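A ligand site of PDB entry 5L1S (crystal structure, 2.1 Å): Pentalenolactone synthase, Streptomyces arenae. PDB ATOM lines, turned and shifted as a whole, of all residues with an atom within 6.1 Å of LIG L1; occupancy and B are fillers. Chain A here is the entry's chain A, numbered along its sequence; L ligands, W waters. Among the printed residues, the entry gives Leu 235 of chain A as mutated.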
ATOM      1  N   ARG A  77      29.948  12.243  11.879  1.00  0.00           N
ATOM      2  CA  ARG A  77      30.453  12.545  13.225  1.00  0.00           C
ATOM      3  C   ARG A  77      31.511  13.639  13.192  1.00  0.00           C
ATOM      4  O   ARG A  77      31.595  14.449  14.131  1.00  0.00           O
ATOM      5  CB  ARG A  77      31.031  11.275  13.869  1.00  0.00           C
ATOM      6  CG  ARG A  77      29.994  10.346  14.465  1.00  0.00           C
ATOM      7  CD  ARG A  77      29.409  10.950  15.743  1.00  0.00           C
ATOM      8  NE  ARG A  77      28.392  10.096  16.340  1.00  0.00           N
ATOM      9  CZ  ARG A  77      27.645  10.444  17.377  1.00  0.00           C
ATOM     10  NH1 ARG A  77      27.779  11.638  17.944  1.00  0.00           N
ATOM     11  NH2 ARG A  77      26.748   9.592  17.852  1.00  0.00           N
ATOM     12  N   MET A  80      29.663  16.922  12.987  1.00  0.00           N
ATOM     13  CA  MET A  80      29.009  17.240  14.253  1.00  0.00           C
ATOM     14  C   MET A  80      30.024  17.768  15.277  1.00  0.00           C
ATOM     15  O   MET A  80      29.758  18.758  15.971  1.00  0.00           O
ATOM     16  CB  MET A  80      28.289  16.006  14.794  1.00  0.00           C
ATOM     17  CG  MET A  80      27.622  16.254  16.147  1.00  0.00           C
ATOM     18  SD  MET A  80      26.407  14.986  16.546  1.00  0.00           S
ATOM     19  CE  MET A  80      25.133  15.390  15.342  1.00  0.00           C
ATOM     20  N   MET A  84      30.514  21.776  16.849  1.00  0.00           N
ATOM     21  CA  MET A  84      30.569  21.982  18.299  1.00  0.00           C
ATOM     22  C   MET A  84      31.953  22.404  18.772  1.00  0.00           C
ATOM     23  O   MET A  84      32.225  22.347  19.989  1.00  0.00           O
ATOM     24  CB  MET A  84      30.129  20.693  19.008  1.00  0.00           C
ATOM     25  CG  MET A  84      28.632  20.392  18.809  1.00  0.00           C
ATOM     26  SD  MET A  84      28.148  18.718  19.282  1.00  0.00           S
ATOM     27  CE  MET A  84      28.254  18.810  21.079  1.00  0.00           C
ATOM     28  N   PHE A 174      24.098  14.172   8.876  1.00  0.00           N
ATOM     29  CA  PHE A 174      24.382  13.231   9.957  1.00  0.00           C
ATOM     30  C   PHE A 174      24.089  11.787   9.575  1.00  0.00           C
ATOM     31  O   PHE A 174      23.867  10.944  10.457  1.00  0.00           O
ATOM     32  CB  PHE A 174      23.627  13.651  11.208  1.00  0.00           C
ATOM     33  CG  PHE A 174      24.012  15.027  11.692  1.00  0.00           C
ATOM     34  CD1 PHE A 174      25.320  15.465  11.593  1.00  0.00           C
ATOM     35  CD2 PHE A 174      23.059  15.882  12.234  1.00  0.00           C
ATOM     36  CE1 PHE A 174      25.693  16.735  12.027  1.00  0.00           C
ATOM     37  CE2 PHE A 174      23.417  17.152  12.664  1.00  0.00           C
ATOM     38  CZ  PHE A 174      24.733  17.584  12.564  1.00  0.00           C
ATOM     39  N   LEU A 234      21.520  23.032  11.955  1.00  0.00           N
ATOM     40  CA  LEU A 234      21.661  21.588  11.950  1.00  0.00           C
ATOM     41  C   LEU A 234      21.351  20.955  13.301  1.00  0.00           C
ATOM     42  O   LEU A 234      20.939  19.791  13.337  1.00  0.00           O
ATOM     43  CB  LEU A 234      23.074  21.179  11.501  1.00  0.00           C
ATOM     44  CG  LEU A 234      23.335  21.384   9.995  1.00  0.00           C
ATOM     45  CD1 LEU A 234      24.840  21.477   9.694  1.00  0.00           C
ATOM     46  CD2 LEU A 234      22.709  20.270   9.175  1.00  0.00           C
ATOM     47  N   LEU A 235      21.492  21.686  14.397  1.00  0.00           N
ATOM     48  CA  LEU A 235      21.101  21.171  15.711  1.00  0.00           C
ATOM     49  C   LEU A 235      19.735  21.691  16.163  1.00  0.00           C
ATOM     50  O   LEU A 235      19.173  21.150  17.128  1.00  0.00           O
ATOM     51  CB  LEU A 235      22.156  21.529  16.768  1.00  0.00           C
ATOM     52  CG  LEU A 235      23.629  21.309  16.344  1.00  0.00           C
ATOM     53  CD1 LEU A 235      24.610  21.622  17.464  1.00  0.00           C
ATOM     54  CD2 LEU A 235      23.877  19.904  15.767  1.00  0.00           C
ATOM     55  N   THR A 239      16.249  17.216  16.280  1.00  0.00           N
ATOM     56  CA  THR A 239      16.024  16.514  17.543  1.00  0.00           C
ATOM     57  C   THR A 239      14.682  16.875  18.171  1.00  0.00           C
ATOM     58  O   THR A 239      14.075  16.042  18.846  1.00  0.00           O
ATOM     59  CB  THR A 239      17.154  16.800  18.544  1.00  0.00           C
ATOM     60  OG1 THR A 239      17.234  18.211  18.796  1.00  0.00           O
ATOM     61  CG2 THR A 239      18.525  16.288  18.015  1.00  0.00           C
ATOM     62  N   ARG A 243      11.495  14.442  19.213  1.00  0.00           N
ATOM     63  CA  ARG A 243      10.796  14.413  20.498  1.00  0.00           C
ATOM     64  C   ARG A 243       9.294  14.604  20.372  1.00  0.00           C
ATOM     65  O   ARG A 243       8.529  14.107  21.217  1.00  0.00           O
ATOM     66  CB  ARG A 243      11.376  15.448  21.474  1.00  0.00           C
ATOM     67  CG  ARG A 243      12.878  15.212  21.797  1.00  0.00           C
ATOM     68  CD  ARG A 243      13.131  13.715  21.931  1.00  0.00           C
ATOM     69  NE  ARG A 243      14.492  13.320  22.283  1.00  0.00           N
ATOM     70  CZ  ARG A 243      15.519  13.311  21.445  1.00  0.00           C
ATOM     71  NH1 ARG A 243      15.396  13.722  20.180  1.00  0.00           N
ATOM     72  NH2 ARG A 243      16.714  12.897  21.875  1.00  0.00           N
ATOM     73  N   SER A 285      21.130   4.851  20.077  1.00  0.00           N
ATOM     74  CA  SER A 285      22.515   5.284  19.936  1.00  0.00           C
ATOM     75  C   SER A 285      22.658   6.793  20.047  1.00  0.00           C
ATOM     76  O   SER A 285      23.758   7.290  20.315  1.00  0.00           O
ATOM     77  CB  SER A 285      23.111   4.824  18.600  1.00  0.00           C
ATOM     78  OG  SER A 285      23.136   3.398  18.506  1.00  0.00           O
ATOM     79  N   ASN A 286      21.569   7.544  19.842  1.00  0.00           N
ATOM     80  CA  ASN A 286      21.603   8.980  20.015  1.00  0.00           C
ATOM     81  C   ASN A 286      21.463   9.395  21.462  1.00  0.00           C
ATOM     82  O   ASN A 286      21.725  10.560  21.799  1.00  0.00           O
ATOM     83  CB  ASN A 286      20.481   9.633  19.175  1.00  0.00           C
ATOM     84  CG  ASN A 286      19.106   9.196  19.609  1.00  0.00           C
ATOM     85  OD1 ASN A 286      18.831   8.001  19.767  1.00  0.00           O
ATOM     86  ND2 ASN A 286      18.227  10.174  19.828  1.00  0.00           N
ATOM     87  N   ALA A 287      21.058   8.478  22.351  1.00  0.00           N
ATOM     88  CA  ALA A 287      20.976   8.757  23.784  1.00  0.00           C
ATOM     89  C   ALA A 287      22.297   8.460  24.497  1.00  0.00           C
ATOM     90  O   ALA A 287      22.294   8.085  25.681  1.00  0.00           O
ATOM     91  CB  ALA A 287      19.834   7.962  24.429  1.00  0.00           C
ATOM     92  N   LEU A 288      23.412   8.588  23.780  1.00  0.00           N
ATOM     93  CA  LEU A 288      24.747   8.445  24.337  1.00  0.00           C
ATOM     94  C   LEU A 288      25.514   9.720  24.029  1.00  0.00           C
ATOM     95  O   LEU A 288      25.536  10.163  22.875  1.00  0.00           O
ATOM     96  CB  LEU A 288      25.475   7.243  23.722  1.00  0.00           C
ATOM     97  CG  LEU A 288      24.814   5.859  23.809  1.00  0.00           C
ATOM     98  CD1 LEU A 288      25.649   4.855  23.015  1.00  0.00           C
ATOM     99  CD2 LEU A 288      24.705   5.432  25.264  1.00  0.00           C
ATOM    100  N   ILE A 289      26.119  10.329  25.043  1.00  0.00           N
ATOM    101  CA  ILE A 289      26.934  11.521  24.865  1.00  0.00           C
ATOM    102  C   ILE A 289      28.390  11.072  24.837  1.00  0.00           C
ATOM    103  O   ILE A 289      28.882  10.521  25.835  1.00  0.00           O
ATOM    104  CB  ILE A 289      26.710  12.552  25.978  1.00  0.00           C
ATOM    105  CG1 ILE A 289      25.301  13.180  25.860  1.00  0.00           C
ATOM    106  CG2 ILE A 289      27.844  13.597  25.938  1.00  0.00           C
ATOM    107  CD1 ILE A 289      25.005  14.293  26.930  1.00  0.00           C
ATOM    108  N   PRO A 290      29.111  11.274  23.724  1.00  0.00           N
ATOM    109  CA  PRO A 290      30.465  10.740  23.623  1.00  0.00           C
ATOM    110  C   PRO A 290      31.492  11.722  24.189  1.00  0.00           C
ATOM    111  O   PRO A 290      31.347  12.941  24.068  1.00  0.00           O
ATOM    112  CB  PRO A 290      30.638  10.549  22.109  1.00  0.00           C
ATOM    113  CG  PRO A 290      29.833  11.706  21.533  1.00  0.00           C
ATOM    114  CD  PRO A 290      28.714  12.013  22.514  1.00  0.00           C
ATOM    115  N   ILE A 314      22.873   8.909  28.727  1.00  0.00           N
ATOM    116  CA  ILE A 314      21.842   9.753  29.314  1.00  0.00           C
ATOM    117  C   ILE A 314      20.472   9.077  29.231  1.00  0.00           C
ATOM    118  O   ILE A 314      19.643   9.232  30.129  1.00  0.00           O
ATOM    119  CB  ILE A 314      21.829  11.144  28.619  1.00  0.00           C
ATOM    120  CG1 ILE A 314      21.606  11.017  27.101  1.00  0.00           C
ATOM    121  CG2 ILE A 314      23.133  11.931  28.935  1.00  0.00           C
ATOM    122  CD1 ILE A 314      21.481  12.369  26.369  1.00  0.00           C
ATOM    123  N   ALA A 342      18.294  14.566  29.488  1.00  0.00           N
ATOM    124  CA  ALA A 342      18.087  14.530  28.035  1.00  0.00           C
ATOM    125  C   ALA A 342      18.684  15.728  27.303  1.00  0.00           C
ATOM    126  O   ALA A 342      18.922  15.638  26.084  1.00  0.00           O
ATOM    127  CB  ALA A 342      16.601  14.426  27.691  1.00  0.00           C
ATOM    128  N   ILE A 390      22.764   9.942  13.021  1.00  0.00           N
ATOM    129  CA  ILE A 390      23.189  10.252  14.387  1.00  0.00           C
ATOM    130  C   ILE A 390      21.990  10.597  15.251  1.00  0.00           C
ATOM    131  O   ILE A 390      21.889  10.166  16.403  1.00  0.00           O
ATOM    132  CB  ILE A 390      24.229  11.397  14.390  1.00  0.00           C
ATOM    133  CG1 ILE A 390      25.530  10.964  13.700  1.00  0.00           C
ATOM    134  CG2 ILE A 390      24.514  11.822  15.831  1.00  0.00           C
ATOM    135  CD1 ILE A 390      26.498  12.115  13.479  1.00  0.00           C
ATOM    136  N   THR A 391      21.030  11.335  14.673  1.00  0.00           N
ATOM    137  CA  THR A 391      19.832  11.765  15.387  1.00  0.00           C
ATOM    138  C   THR A 391      18.673  10.767  15.294  1.00  0.00           C
ATOM    139  O   THR A 391      17.579  11.073  15.766  1.00  0.00           O
ATOM    140  CB  THR A 391      19.395  13.143  14.861  1.00  0.00           C
ATOM    141  OG1 THR A 391      19.482  13.154  13.426  1.00  0.00           O
ATOM    142  CG2 THR A 391      20.303  14.243  15.392  1.00  0.00           C
ATOM    143  N   GLY A 392      18.882   9.580  14.700  1.00  0.00           N
ATOM    144  CA  GLY A 392      17.841   8.559  14.659  1.00  0.00           C
ATOM    145  C   GLY A 392      16.528   9.057  14.060  1.00  0.00           C
ATOM    146  O   GLY A 392      16.505   9.642  12.975  1.00  0.00           O
HETATM  147  C1  LIG L   1      22.585  17.045  20.776  1.00  0.00           C
HETATM  148  C2  LIG L   1      23.384  17.111  19.467  1.00  0.00           C
HETATM  149  C3  LIG L   1      24.277  18.348  19.462  1.00  0.00           C
HETATM  150  C4  LIG L   1      22.472  17.171  18.209  1.00  0.00           C
HETATM  151  C5  LIG L   1      21.246  14.905  21.082  1.00  0.00           C
HETATM  152  C6  LIG L   1      22.830  12.602  19.134  1.00  0.00           C
HETATM  153  C7  LIG L   1      23.887  13.113  22.289  1.00  0.00           C
HETATM  154  C8  LIG L   1      24.283  15.853  19.566  1.00  0.00           C
HETATM  155  C9  LIG L   1      20.027  13.406  19.645  1.00  0.00           C
HETATM  156  C10 LIG L   1      25.045  12.959  20.068  1.00  0.00           C
HETATM  157  C11 LIG L   1      21.147  14.131  19.974  1.00  0.00           C
HETATM  158  C12 LIG L   1      22.534  15.543  21.229  1.00  0.00           C
HETATM  159  C13 LIG L   1      22.386  14.099  19.281  1.00  0.00           C
HETATM  160  C14 LIG L   1      24.312  13.738  20.974  1.00  0.00           C
HETATM  161  C15 LIG L   1      23.400  14.776  20.235  1.00  0.00           C
HETATM  162  O1  LIG L   1      19.028  13.370  20.407  1.00  0.00           O
HETATM  163  O2  LIG L   1      26.277  12.839  20.156  1.00  0.00           O
HETATM  164  O3  LIG L   1      19.920  12.760  18.581  1.00  0.00           O
HETATM  165  O4  LIG L   1      24.314  12.402  19.052  1.00  0.00           O
HETATM  166  O5  LIG L   1      24.946  14.118  22.208  1.00  0.00           O
HETATM  167  C1  LG2 L   2      23.713  20.441  22.857  1.00  0.00           C
HETATM  168  C2  LG2 L   2      19.770  17.633  23.317  1.00  0.00           C
HETATM  169  C3  LG2 L   2      17.168  20.964  20.926  1.00  0.00           C
HETATM  170  C4  LG2 L   2      21.133  23.664  20.260  1.00  0.00           C
HETATM  171  C5  LG2 L   2      22.880  19.410  23.249  1.00  0.00           C
HETATM  172  C6  LG2 L   2      23.248  18.272  24.067  1.00  0.00           C
HETATM  173  C7  LG2 L   2      22.149  17.487  24.189  1.00  0.00           C
HETATM  174  C8  LG2 L   2      21.056  18.120  23.462  1.00  0.00           C
HETATM  175  C9  LG2 L   2      22.019  16.145  24.946  1.00  0.00           C
HETATM  176  C10 LG2 L   2      24.648  18.033  24.691  1.00  0.00           C
HETATM  177  C11 LG2 L   2      25.602  17.344  23.715  1.00  0.00           C
HETATM  178  C12 LG2 L   2      26.905  16.993  24.417  1.00  0.00           C
HETATM  179  O1  LG2 L   2      27.015  17.201  25.660  1.00  0.00           O
HETATM  180  O2  LG2 L   2      27.836  16.508  23.724  1.00  0.00           O
HETATM  181  C13 LG2 L   2      18.707  18.262  22.700  1.00  0.00           C
HETATM  182  C14 LG2 L   2      17.335  17.796  22.628  1.00  0.00           C
HETATM  183  C15 LG2 L   2      16.630  18.742  21.948  1.00  0.00           C
HETATM  184  C16 LG2 L   2      17.534  19.821  21.612  1.00  0.00           C
HETATM  185  C17 LG2 L   2      16.793  16.456  23.201  1.00  0.00           C
HETATM  186  C18 LG2 L   2      15.128  18.788  21.589  1.00  0.00           C
HETATM  187  C19 LG2 L   2      14.173  18.316  22.401  1.00  0.00           C
HETATM  188  C20 LG2 L   2      17.979  22.027  20.559  1.00  0.00           C
HETATM  189  C21 LG2 L   2      17.550  23.271  19.937  1.00  0.00           C
HETATM  190  C22 LG2 L   2      18.663  24.020  19.763  1.00  0.00           C
HETATM  191  C23 LG2 L   2      19.809  23.264  20.248  1.00  0.00           C
HETATM  192  C24 LG2 L   2      16.065  23.585  19.591  1.00  0.00           C
HETATM  193  C25 LG2 L   2      18.816  25.430  19.132  1.00  0.00           C
HETATM  194  C26 LG2 L   2      17.876  26.045  18.409  1.00  0.00           C
HETATM  195  C27 LG2 L   2      22.181  22.986  20.858  1.00  0.00           C
HETATM  196  C28 LG2 L   2      23.582  23.348  20.751  1.00  0.00           C
HETATM  197  C29 LG2 L   2      24.292  22.452  21.460  1.00  0.00           C
HETATM  198  C30 LG2 L   2      23.372  21.496  22.036  1.00  0.00           C
HETATM  199  C31 LG2 L   2      24.109  24.555  19.948  1.00  0.00           C
HETATM  200  C32 LG2 L   2      25.815  22.421  21.657  1.00  0.00           C
HETATM  201  C33 LG2 L   2      26.124  22.990  23.044  1.00  0.00           C
HETATM  202  C34 LG2 L   2      27.615  22.896  23.338  1.00  0.00           C
HETATM  203  O3  LG2 L   2      28.113  23.662  24.214  1.00  0.00           O
HETATM  204  O4  LG2 L   2      28.309  22.077  22.670  1.00  0.00           O
HETATM  205  N1  LG2 L   2      21.543  19.287  22.896  1.00  0.00           N
HETATM  206  N2  LG2 L   2      18.785  19.492  22.068  1.00  0.00           N
HETATM  207  N3  LG2 L   2      19.351  22.069  20.736  1.00  0.00           N
HETATM  208  N4  LG2 L   2      22.110  21.863  21.645  1.00  0.00           N
HETATM  209 FE1  LG2 L   2      20.376  20.817  22.039  1.00  0.00          FE
HETATM  210  O   HOH W   1      20.024  12.534  22.987  1.00  0.00           O
HETATM  211  O   HOH W   2      27.876  15.002  21.378  1.00  0.00           O
HETATM  212  O   HOH W   3      17.138  12.852  17.965  1.00  0.00           O
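The side-chain amide nitrogen of Asn 286 lies close to an oxygen (O3) of LIG L1 (3.3 Å).
An oxygen (O2) of LIG L1 sits at hydrogen-bond distance from the guanidinium group (NH1) of Arg 77, at 2.9 Å.
O1 of LIG L1 is in salt-bridge range of NH2 of Arg 243, 2.8 Å away.
The backbone NH (N) of Ile 390 lies within hydrogen-bond range of the backbone carbonyl oxygen (O) of Phe 174.
O of Thr 239 lies within hydrogen-bond range of NH1 of Arg 243, at 3.0 Å.
Water W3 lies within hydrogen-bond range of O3 of LIG L1 (2.9 Å), O of Thr 391 (2.9 Å), NH1 of Arg 243 (2.9 Å) and ND2 of Asn 286 (3.4 Å).
Water W1 bridges the backbone carbonyl oxygen of Asn 286 (2.9 Å) and an oxygen (O1) of LIG L1 (2.9 Å).
Water W2 bridges an oxygen (O2) of LG2 L2 (2.8 Å) and an oxygen (O2) of LIG L1 (3.0 Å).
Met 80 touches LIG L1.
SD of Met 84 touches C3 of LIG L1, at 3.9 Å.
CD1 of Leu 235 touches C3 of LIG L1 (3.8 Å).
CG2 of Thr 239 touches C9 of LIG L1, 3.6 Å away.
Leu 288 touches LIG L1 (O to C7, 3.4 Å).
Ile 289 touches LIG L1.
Pro 290 touches LIG L1.
Ile 390 touches LIG L1 (CG2 to O4, 3.3 Å).
CA of Thr 391 touches O3 of LIG L1 (3.3 Å).
Hydrophobic or aromatic side chains within 4 Å of LIG L1: Met 80, Met 84, Leu 235, Ile 289, Pro 290 and Ile 390.
Within 4 Å of LIG L1: Arg 77, Met 80, Met 84, Leu 235, Thr 239, Arg 243, Asn 286, Leu 288, Ile 289, Pro 290, Ile 390 and Thr 391.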
